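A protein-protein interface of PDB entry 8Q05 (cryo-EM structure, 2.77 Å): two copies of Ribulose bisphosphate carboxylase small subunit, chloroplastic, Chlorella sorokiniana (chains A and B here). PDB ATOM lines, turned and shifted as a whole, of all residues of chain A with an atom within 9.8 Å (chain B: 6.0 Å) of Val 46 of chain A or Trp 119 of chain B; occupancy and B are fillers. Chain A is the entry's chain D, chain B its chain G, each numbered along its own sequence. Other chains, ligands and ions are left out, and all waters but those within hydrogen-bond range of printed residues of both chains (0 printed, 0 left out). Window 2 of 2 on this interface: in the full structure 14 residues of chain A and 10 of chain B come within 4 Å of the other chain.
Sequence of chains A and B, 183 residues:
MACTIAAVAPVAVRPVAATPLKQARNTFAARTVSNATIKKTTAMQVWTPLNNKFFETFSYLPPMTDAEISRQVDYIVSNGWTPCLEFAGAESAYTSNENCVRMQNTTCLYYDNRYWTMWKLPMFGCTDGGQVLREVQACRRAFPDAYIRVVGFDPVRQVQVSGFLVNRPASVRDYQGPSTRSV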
ATOM      1  N   GLN A  45     -33.145 -15.547   9.326  1.00  0.00           N
ATOM      2  CA  GLN A  45     -31.946 -16.389   9.064  1.00  0.00           C
ATOM      3  C   GLN A  45     -32.301 -17.856   9.315  1.00  0.00           C
ATOM      4  O   GLN A  45     -33.325 -18.107   9.978  1.00  0.00           O
ATOM      5  CB  GLN A  45     -30.763 -15.946   9.922  1.00  0.00           C
ATOM      6  CG  GLN A  45     -29.500 -15.724   9.107  1.00  0.00           C
ATOM      7  CD  GLN A  45     -29.720 -14.679   8.042  1.00  0.00           C
ATOM      8  OE1 GLN A  45     -30.057 -13.533   8.333  1.00  0.00           O
ATOM      9  NE2 GLN A  45     -29.535 -15.069   6.792  1.00  0.00           N
ATOM     10  N   VAL A  46     -31.489 -18.782   8.801  1.00  0.00           N
ATOM     11  CA  VAL A  46     -31.819 -20.233   8.927  1.00  0.00           C
ATOM     12  C   VAL A  46     -30.674 -20.968   9.627  1.00  0.00           C
ATOM     13  O   VAL A  46     -29.536 -20.894   9.123  1.00  0.00           O
ATOM     14  CB  VAL A  46     -32.120 -20.858   7.549  1.00  0.00           C
ATOM     15  CG1 VAL A  46     -32.270 -22.368   7.634  1.00  0.00           C
ATOM     16  CG2 VAL A  46     -33.344 -20.232   6.900  1.00  0.00           C
ATOM     17  N   TRP A  47     -30.965 -21.644  10.741  1.00  0.00           N
ATOM     18  CA  TRP A  47     -29.938 -22.464  11.434  1.00  0.00           C
ATOM     19  C   TRP A  47     -29.329 -23.431  10.416  1.00  0.00           C
ATOM     20  O   TRP A  47     -30.100 -24.185   9.799  1.00  0.00           O
ATOM     21  CB  TRP A  47     -30.568 -23.213  12.611  1.00  0.00           C
ATOM     22  CG  TRP A  47     -29.585 -23.793  13.581  1.00  0.00           C
ATOM     23  CD1 TRP A  47     -29.345 -25.115  13.818  1.00  0.00           C
ATOM     24  CD2 TRP A  47     -28.732 -23.064  14.481  1.00  0.00           C
ATOM     25  NE1 TRP A  47     -28.390 -25.259  14.786  1.00  0.00           N
ATOM     26  CE2 TRP A  47     -27.996 -24.018  15.213  1.00  0.00           C
ATOM     27  CE3 TRP A  47     -28.513 -21.705  14.734  1.00  0.00           C
ATOM     28  CZ2 TRP A  47     -27.059 -23.654  16.179  1.00  0.00           C
ATOM     29  CZ3 TRP A  47     -27.587 -21.346  15.688  1.00  0.00           C
ATOM     30  CH2 TRP A  47     -26.871 -22.309  16.399  1.00  0.00           C
ATOM     31  N   THR A  48     -28.009 -23.395  10.232  1.00  0.00           N
ATOM     32  CA  THR A  48     -27.367 -24.246   9.193  1.00  0.00           C
ATOM     33  C   THR A  48     -27.322 -25.702   9.667  1.00  0.00           C
ATOM     34  O   THR A  48     -26.946 -25.935  10.832  1.00  0.00           O
ATOM     35  CB  THR A  48     -25.978 -23.726   8.796  1.00  0.00           C
ATOM     36  OG1 THR A  48     -25.478 -24.581   7.767  1.00  0.00           O
ATOM     37  CG2 THR A  48     -24.994 -23.687   9.945  1.00  0.00           C
ATOM     38  N   PRO A  49     -27.757 -26.703   8.862  1.00  0.00           N
ATOM     39  CA  PRO A  49     -27.643 -28.106   9.254  1.00  0.00           C
ATOM     40  C   PRO A  49     -26.365 -28.731   8.687  1.00  0.00           C
ATOM     41  O   PRO A  49     -26.215 -29.933   8.785  1.00  0.00           O
ATOM     42  CB  PRO A  49     -28.866 -28.721   8.567  1.00  0.00           C
ATOM     43  CG  PRO A  49     -28.952 -27.973   7.257  1.00  0.00           C
ATOM     44  CD  PRO A  49     -28.437 -26.580   7.560  1.00  0.00           C
ATOM     45  N   LEU A  50     -25.483 -27.908   8.113  1.00  0.00           N
ATOM     46  CA  LEU A  50     -24.250 -28.438   7.470  1.00  0.00           C
ATOM     47  C   LEU A  50     -23.037 -28.115   8.347  1.00  0.00           C
ATOM     48  O   LEU A  50     -22.847 -26.927   8.670  1.00  0.00           O
ATOM     49  CB  LEU A  50     -24.107 -27.803   6.085  1.00  0.00           C
ATOM     50  CG  LEU A  50     -25.251 -28.085   5.112  1.00  0.00           C
ATOM     51  CD1 LEU A  50     -24.912 -27.580   3.719  1.00  0.00           C
ATOM     52  CD2 LEU A  50     -25.571 -29.572   5.073  1.00  0.00           C
ATOM     53  N   ASN A  52     -22.391 -28.339  11.484  1.00  0.00           N
ATOM     54  CA  ASN A  52     -22.735 -27.547  12.693  1.00  0.00           C
ATOM     55  C   ASN A  52     -22.838 -28.502  13.887  1.00  0.00           C
ATOM     56  O   ASN A  52     -23.936 -28.611  14.461  1.00  0.00           O
ATOM     57  CB  ASN A  52     -24.016 -26.733  12.493  1.00  0.00           C
ATOM     58  CG  ASN A  52     -24.061 -25.480  13.339  1.00  0.00           C
ATOM     59  OD1 ASN A  52     -23.106 -25.172  14.049  1.00  0.00           O
ATOM     60  ND2 ASN A  52     -25.158 -24.745  13.262  1.00  0.00           N
ATOM     61  N   GLN A 176     -19.407 -25.036  13.176  1.00  0.00           N
ATOM     62  CA  GLN A 176     -19.507 -23.661  12.617  1.00  0.00           C
ATOM     63  C   GLN A 176     -18.976 -22.652  13.636  1.00  0.00           C
ATOM     64  O   GLN A 176     -18.498 -23.086  14.702  1.00  0.00           O
ATOM     65  CB  GLN A 176     -20.959 -23.312  12.288  1.00  0.00           C
ATOM     66  CG  GLN A 176     -21.538 -24.099  11.125  1.00  0.00           C
ATOM     67  CD  GLN A 176     -20.807 -23.836   9.832  1.00  0.00           C
ATOM     68  OE1 GLN A 176     -20.738 -22.707   9.354  1.00  0.00           O
ATOM     69  NE2 GLN A 176     -20.251 -24.887   9.252  1.00  0.00           N
ATOM     70  N   SER A 179     -21.065 -16.716  14.235  1.00  0.00           N
ATOM     71  CA  SER A 179     -21.762 -15.922  13.187  1.00  0.00           C
ATOM     72  C   SER A 179     -22.156 -16.812  12.002  1.00  0.00           C
ATOM     73  O   SER A 179     -23.056 -16.406  11.241  1.00  0.00           O
ATOM     74  CB  SER A 179     -20.903 -14.772  12.733  1.00  0.00           C
ATOM     75  OG  SER A 179     -19.730 -15.246  12.088  1.00  0.00           O
ATOM     76  N   THR A 180     -21.509 -17.971  11.846  1.00  0.00           N
ATOM     77  CA  THR A 180     -21.780 -18.847  10.673  1.00  0.00           C
ATOM     78  C   THR A 180     -22.802 -19.927  11.047  1.00  0.00           C
ATOM     79  O   THR A 180     -23.097 -20.777  10.186  1.00  0.00           O
ATOM     80  CB  THR A 180     -20.477 -19.450  10.135  1.00  0.00           C
ATOM     81  OG1 THR A 180     -19.970 -20.359  11.112  1.00  0.00           O
ATOM     82  CG2 THR A 180     -19.432 -18.404   9.817  1.00  0.00           C
ATOM     83  N   ARG A 181     -23.327 -19.882  12.274  1.00  0.00           N
ATOM     84  CA  ARG A 181     -24.331 -20.879  12.733  1.00  0.00           C
ATOM     85  C   ARG A 181     -25.667 -20.627  12.025  1.00  0.00           C
ATOM     86  O   ARG A 181     -26.468 -21.577  11.930  1.00  0.00           O
ATOM     87  CB  ARG A 181     -24.482 -20.800  14.254  1.00  0.00           C
ATOM     88  CG  ARG A 181     -23.320 -21.404  15.025  1.00  0.00           C
ATOM     89  CD  ARG A 181     -23.292 -20.929  16.464  1.00  0.00           C
ATOM     90  NE  ARG A 181     -22.131 -21.425  17.190  1.00  0.00           N
ATOM     91  CZ  ARG A 181     -21.839 -21.105  18.444  1.00  0.00           C
ATOM     92  NH1 ARG A 181     -22.495 -20.127  19.044  1.00  0.00           N
ATOM     93  NH2 ARG A 181     -20.889 -21.757  19.091  1.00  0.00           N
ATOM     94  N   SER A 182     -25.899 -19.397  11.558  1.00  0.00           N
ATOM     95  CA  SER A 182     -27.142 -19.083  10.804  1.00  0.00           C
ATOM     96  C   SER A 182     -26.789 -18.558   9.409  1.00  0.00           C
ATOM     97  O   SER A 182     -25.831 -17.766   9.304  1.00  0.00           O
ATOM     98  CB  SER A 182     -28.008 -18.111  11.559  1.00  0.00           C
ATOM     99  OG  SER A 182     -28.613 -18.743  12.677  1.00  0.00           O
ATOM    100  N   VAL A 183     -27.531 -18.986   8.383  1.00  0.00           N
ATOM    101  CA  VAL A 183     -27.237 -18.573   6.977  1.00  0.00           C
ATOM    102  C   VAL A 183     -28.524 -18.044   6.334  1.00  0.00           C
ATOM    103  O   VAL A 183     -29.554 -18.045   7.033  1.00  0.00           O
ATOM    104  CB  VAL A 183     -26.645 -19.741   6.166  1.00  0.00           C
ATOM    105  CG1 VAL A 183     -26.454 -19.372   4.703  1.00  0.00           C
ATOM    106  CG2 VAL A 183     -25.342 -20.245   6.767  1.00  0.00           C
ATOM    107  N   LEU B  85     -40.328 -24.138   1.894  1.00  0.00           N
ATOM    108  CA  LEU B  85     -39.180 -24.714   1.154  1.00  0.00           C
ATOM    109  C   LEU B  85     -38.400 -25.682   2.037  1.00  0.00           C
ATOM    110  O   LEU B  85     -38.121 -25.336   3.197  1.00  0.00           O
ATOM    111  CB  LEU B  85     -38.266 -23.570   0.712  1.00  0.00           C
ATOM    112  CG  LEU B  85     -38.760 -22.749  -0.473  1.00  0.00           C
ATOM    113  CD1 LEU B  85     -37.685 -21.774  -0.914  1.00  0.00           C
ATOM    114  CD2 LEU B  85     -39.154 -23.662  -1.620  1.00  0.00           C
ATOM    115  N   GLU B  86     -38.085 -26.855   1.484  1.00  0.00           N
ATOM    116  CA  GLU B  86     -37.237 -27.836   2.201  1.00  0.00           C
ATOM    117  C   GLU B  86     -35.942 -27.974   1.407  1.00  0.00           C
ATOM    118  O   GLU B  86     -35.989 -27.816   0.177  1.00  0.00           O
ATOM    119  CB  GLU B  86     -37.890 -29.214   2.254  1.00  0.00           C
ATOM    120  CG  GLU B  86     -39.080 -29.316   3.183  1.00  0.00           C
ATOM    121  CD  GLU B  86     -39.627 -30.732   3.228  1.00  0.00           C
ATOM    122  OE1 GLU B  86     -39.040 -31.607   2.566  1.00  0.00           O
ATOM    123  OE2 GLU B  86     -40.644 -30.952   3.905  1.00  0.00           O
ATOM    124  N   PHE B  87     -34.837 -28.258   2.084  1.00  0.00           N
ATOM    125  CA  PHE B  87     -33.555 -28.445   1.426  1.00  0.00           C
ATOM    126  C   PHE B  87     -32.748 -29.500   2.163  1.00  0.00           C
ATOM    127  O   PHE B  87     -32.872 -29.662   3.378  1.00  0.00           O
ATOM    128  CB  PHE B  87     -32.767 -27.129   1.343  1.00  0.00           C
ATOM    129  CG  PHE B  87     -32.398 -26.561   2.677  1.00  0.00           C
ATOM    130  CD1 PHE B  87     -33.315 -25.832   3.409  1.00  0.00           C
ATOM    131  CD2 PHE B  87     -31.136 -26.756   3.203  1.00  0.00           C
ATOM    132  CE1 PHE B  87     -32.979 -25.311   4.639  1.00  0.00           C
ATOM    133  CE2 PHE B  87     -30.796 -26.239   4.429  1.00  0.00           C
ATOM    134  CZ  PHE B  87     -31.718 -25.512   5.147  1.00  0.00           C
ATOM    135  N   THR B 117     -34.880 -30.248   5.780  1.00  0.00           N
ATOM    136  CA  THR B 117     -34.760 -29.087   6.700  1.00  0.00           C
ATOM    137  C   THR B 117     -35.592 -27.925   6.155  1.00  0.00           C
ATOM    138  O   THR B 117     -35.467 -27.625   4.956  1.00  0.00           O
ATOM    139  CB  THR B 117     -33.291 -28.693   6.903  1.00  0.00           C
ATOM    140  OG1 THR B 117     -32.580 -29.854   7.333  1.00  0.00           O
ATOM    141  CG2 THR B 117     -33.115 -27.579   7.911  1.00  0.00           C
ATOM    142  N   MET B 118     -36.407 -27.302   7.008  1.00  0.00           N
ATOM    143  CA  MET B 118     -37.265 -26.169   6.570  1.00  0.00           C
ATOM    144  C   MET B 118     -36.391 -24.949   6.269  1.00  0.00           C
ATOM    145  O   MET B 118     -35.394 -24.745   6.986  1.00  0.00           O
ATOM    146  CB  MET B 118     -38.284 -25.811   7.655  1.00  0.00           C
ATOM    147  CG  MET B 118     -39.620 -26.502   7.479  1.00  0.00           C
ATOM    148  SD  MET B 118     -40.593 -25.777   6.138  1.00  0.00           S
ATOM    149  CE  MET B 118     -40.180 -24.045   6.333  1.00  0.00           C
ATOM    150  N   TRP B 119     -36.751 -24.186   5.237  1.00  0.00           N
ATOM    151  CA  TRP B 119     -35.962 -22.988   4.850  1.00  0.00           C
ATOM    152  C   TRP B 119     -36.689 -21.727   5.328  1.00  0.00           C
ATOM    153  O   TRP B 119     -36.656 -21.483   6.549  1.00  0.00           O
ATOM    154  CB  TRP B 119     -35.732 -22.974   3.335  1.00  0.00           C
ATOM    155  CG  TRP B 119     -35.228 -21.668   2.807  1.00  0.00           C
ATOM    156  CD1 TRP B 119     -35.941 -20.726   2.125  1.00  0.00           C
ATOM    157  CD2 TRP B 119     -33.887 -21.157   2.915  1.00  0.00           C
ATOM    158  NE1 TRP B 119     -35.139 -19.666   1.803  1.00  0.00           N
ATOM    159  CE2 TRP B 119     -33.875 -19.900   2.275  1.00  0.00           C
ATOM    160  CE3 TRP B 119     -32.703 -21.634   3.485  1.00  0.00           C
ATOM    161  CZ2 TRP B 119     -32.725 -19.117   2.194  1.00  0.00           C
ATOM    162  CZ3 TRP B 119     -31.567 -20.862   3.402  1.00  0.00           C
ATOM    163  CH2 TRP B 119     -31.579 -19.622   2.765  1.00  0.00           C
ATOM    164  N   GLU B 135     -37.366 -16.803  -2.423  1.00  0.00           N
ATOM    165  CA  GLU B 135     -36.790 -17.675  -1.407  1.00  0.00           C
ATOM    166  C   GLU B 135     -36.052 -18.854  -2.026  1.00  0.00           C
ATOM    167  O   GLU B 135     -35.066 -19.329  -1.458  1.00  0.00           O
ATOM    168  CB  GLU B 135     -37.878 -18.164  -0.456  1.00  0.00           C
ATOM    169  CG  GLU B 135     -38.122 -17.251   0.733  1.00  0.00           C
ATOM    170  CD  GLU B 135     -36.934 -16.361   1.055  1.00  0.00           C
ATOM    171  OE1 GLU B 135     -37.071 -15.126   0.933  1.00  0.00           O
ATOM    172  OE2 GLU B 135     -35.875 -16.891   1.458  1.00  0.00           O
ATOM    173  N   VAL B 136     -36.514 -19.342  -3.178  1.00  0.00           N
ATOM    174  CA  VAL B 136     -35.817 -20.422  -3.869  1.00  0.00           C
ATOM    175  C   VAL B 136     -34.439 -19.958  -4.324  1.00  0.00           C
ATOM    176  O   VAL B 136     -33.440 -20.664  -4.147  1.00  0.00           O
ATOM    177  CB  VAL B 136     -36.666 -20.937  -5.048  1.00  0.00           C
ATOM    178  CG1 VAL B 136     -35.801 -21.657  -6.063  1.00  0.00           C
ATOM    179  CG2 VAL B 136     -37.769 -21.852  -4.550  1.00  0.00           C
ATOM    180  N   ALA B 138     -32.760 -17.489  -2.956  1.00  0.00           N
ATOM    181  CA  ALA B 138     -31.975 -17.284  -1.744  1.00  0.00           C
ATOM    182  C   ALA B 138     -31.414 -18.601  -1.218  1.00  0.00           C
ATOM    183  O   ALA B 138     -30.244 -18.674  -0.825  1.00  0.00           O
ATOM    184  CB  ALA B 138     -32.826 -16.595  -0.678  1.00  0.00           C
ATOM    185  N   CYS B 139     -32.233 -19.655  -1.208  1.00  0.00           N
ATOM    186  CA  CYS B 139     -31.765 -20.962  -0.763  1.00  0.00           C
ATOM    187  C   CYS B 139     -30.697 -21.509  -1.699  1.00  0.00           C
ATOM    188  O   CYS B 139     -29.728 -22.129  -1.248  1.00  0.00           O
ATOM    189  CB  CYS B 139     -32.940 -21.934  -0.657  1.00  0.00           C
ATOM    190  SG  CYS B 139     -32.586 -23.472   0.225  1.00  0.00           S
ATOM    191  N   ARG B 140     -30.861 -21.289  -3.006  1.00  0.00           N
ATOM    192  CA  ARG B 140     -29.855 -21.710  -3.973  1.00  0.00           C
ATOM    193  C   ARG B 140     -28.518 -21.041  -3.695  1.00  0.00           C
ATOM    194  O   ARG B 140     -27.467 -21.692  -3.709  1.00  0.00           O
ATOM    195  CB  ARG B 140     -30.327 -21.380  -5.389  1.00  0.00           C
ATOM    196  CG  ARG B 140     -30.929 -22.540  -6.148  1.00  0.00           C
ATOM    197  CD  ARG B 140     -31.480 -22.082  -7.486  1.00  0.00           C
ATOM    198  NE  ARG B 140     -32.793 -22.646  -7.770  1.00  0.00           N
ATOM    199  CZ  ARG B 140     -33.522 -22.340  -8.835  1.00  0.00           C
ATOM    200  NH1 ARG B 140     -33.102 -21.462  -9.729  1.00  0.00           N
ATOM    201  NH2 ARG B 140     -34.700 -22.931  -9.008  1.00  0.00           N
ATOM    202  N   ALA B 142     -27.501 -19.688  -0.811  1.00  0.00           N
ATOM    203  CA  ALA B 142     -26.974 -20.067   0.497  1.00  0.00           C
ATOM    204  C   ALA B 142     -26.443 -21.496   0.501  1.00  0.00           C
ATOM    205  O   ALA B 142     -25.389 -21.770   1.088  1.00  0.00           O
ATOM    206  CB  ALA B 142     -28.050 -19.895   1.563  1.00  0.00           C
ATOM    207  N   PHE B 143     -27.184 -22.405  -0.143  1.00  0.00           N
ATOM    208  CA  PHE B 143     -26.779 -23.834  -0.192  1.00  0.00           C
ATOM    209  C   PHE B 143     -26.781 -24.300  -1.650  1.00  0.00           C
ATOM    210  O   PHE B 143     -27.784 -24.893  -2.090  1.00  0.00           O
ATOM    211  CB  PHE B 143     -27.731 -24.681   0.656  1.00  0.00           C
ATOM    212  CG  PHE B 143     -27.889 -24.213   2.080  1.00  0.00           C
ATOM    213  CD1 PHE B 143     -26.831 -24.274   2.970  1.00  0.00           C
ATOM    214  CD2 PHE B 143     -29.092 -23.687   2.523  1.00  0.00           C
ATOM    215  CE1 PHE B 143     -26.975 -23.837   4.276  1.00  0.00           C
ATOM    216  CE2 PHE B 143     -29.234 -23.247   3.829  1.00  0.00           C
ATOM    217  CZ  PHE B 143     -28.177 -23.323   4.704  1.00  0.00           C
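The backbone carbonyl oxygen of Val 183 of chain A lies within hydrogen-bond range of the side-chain amide nitrogen of Gln 45 of chain A, 3.0 Å away.
N of Leu 50 of chain A lies close to OG1 of Thr 48 of chain A (3.3 Å).
The backbone NH of Thr 48 of chain A sits at hydrogen-bond distance from the backbone carbonyl oxygen of Arg 181 of chain A.
O of Leu 50 of chain A is in hydrogen-bond range of NE2 of Gln 176 of chain A, at 3.4 Å.
The backbone NH of Trp 119 of chain B is in hydrogen-bond range of the backbone carbonyl oxygen of Leu 85 of chain B.
The side-chain carboxylate of Glu 135 of chain B lies within hydrogen-bond range of the indole nitrogen of Trp 119 of chain B, at 2.9 Å.
Val 46 of chain A touches Met 118 of chain B (CG1 to O, 3.98 Å).
Trp 119 of chain B touches Val 46 of chain A (O to CG2, 3.6 Å).
Thr 48 of chain A touches Phe 143 of chain B.
CG of Pro 49 of chain A touches CE2 of Phe 87 of chain B (3.8 Å).
Leu 50 of chain A touches Phe 143 of chain B.
Val 183 of chain A touches Ala 142 of chain B (CG1 to CB, 3.6 Å).
Val 46 of chain A touches just these residues of chain B: Met 118 and Trp 119.
Of chain A, only Val 46 (3.98 Å) comes within 4 Å of Met 118 of chain B.
Of the printed residues of chain A, Phe 143 of chain B touches Thr 48 (3.9 Å) and Leu 50 (3.9 Å).
Of the printed residues of chain B, Thr 48 of chain A touches Phe 143.
Trp 47 of chain A touches none of the printed residues of chain B.
Gln 45 of chain A touches none of the printed residues of chain B.
The nearest residue of chain B that does not touch Val 46 of chain A is Phe 87 of chain B (4.05 Å).
The nearest residue of chain A that does not touch Trp 119 of chain B is Val 183 of chain A (5.0 Å).
Of the 13 printed residues of chain A, 5 touch a printed residue of chain B.
Hydrophobic or aromatic side chains of chain A within 4 Å of the printed part of chain B: Val 46, Pro 49, Leu 50 and Val 183.
Hydrophobic or aromatic side chains of chain B within 4 Å of the printed part of chain A: Phe 87, Trp 119, Ala 142 and Phe 143.
Among the printed residues, no Asp or Glu carboxylate lies within 4 Å of a Lys or Arg side-chain nitrogen of the other chain.
No position is printed for both chains.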
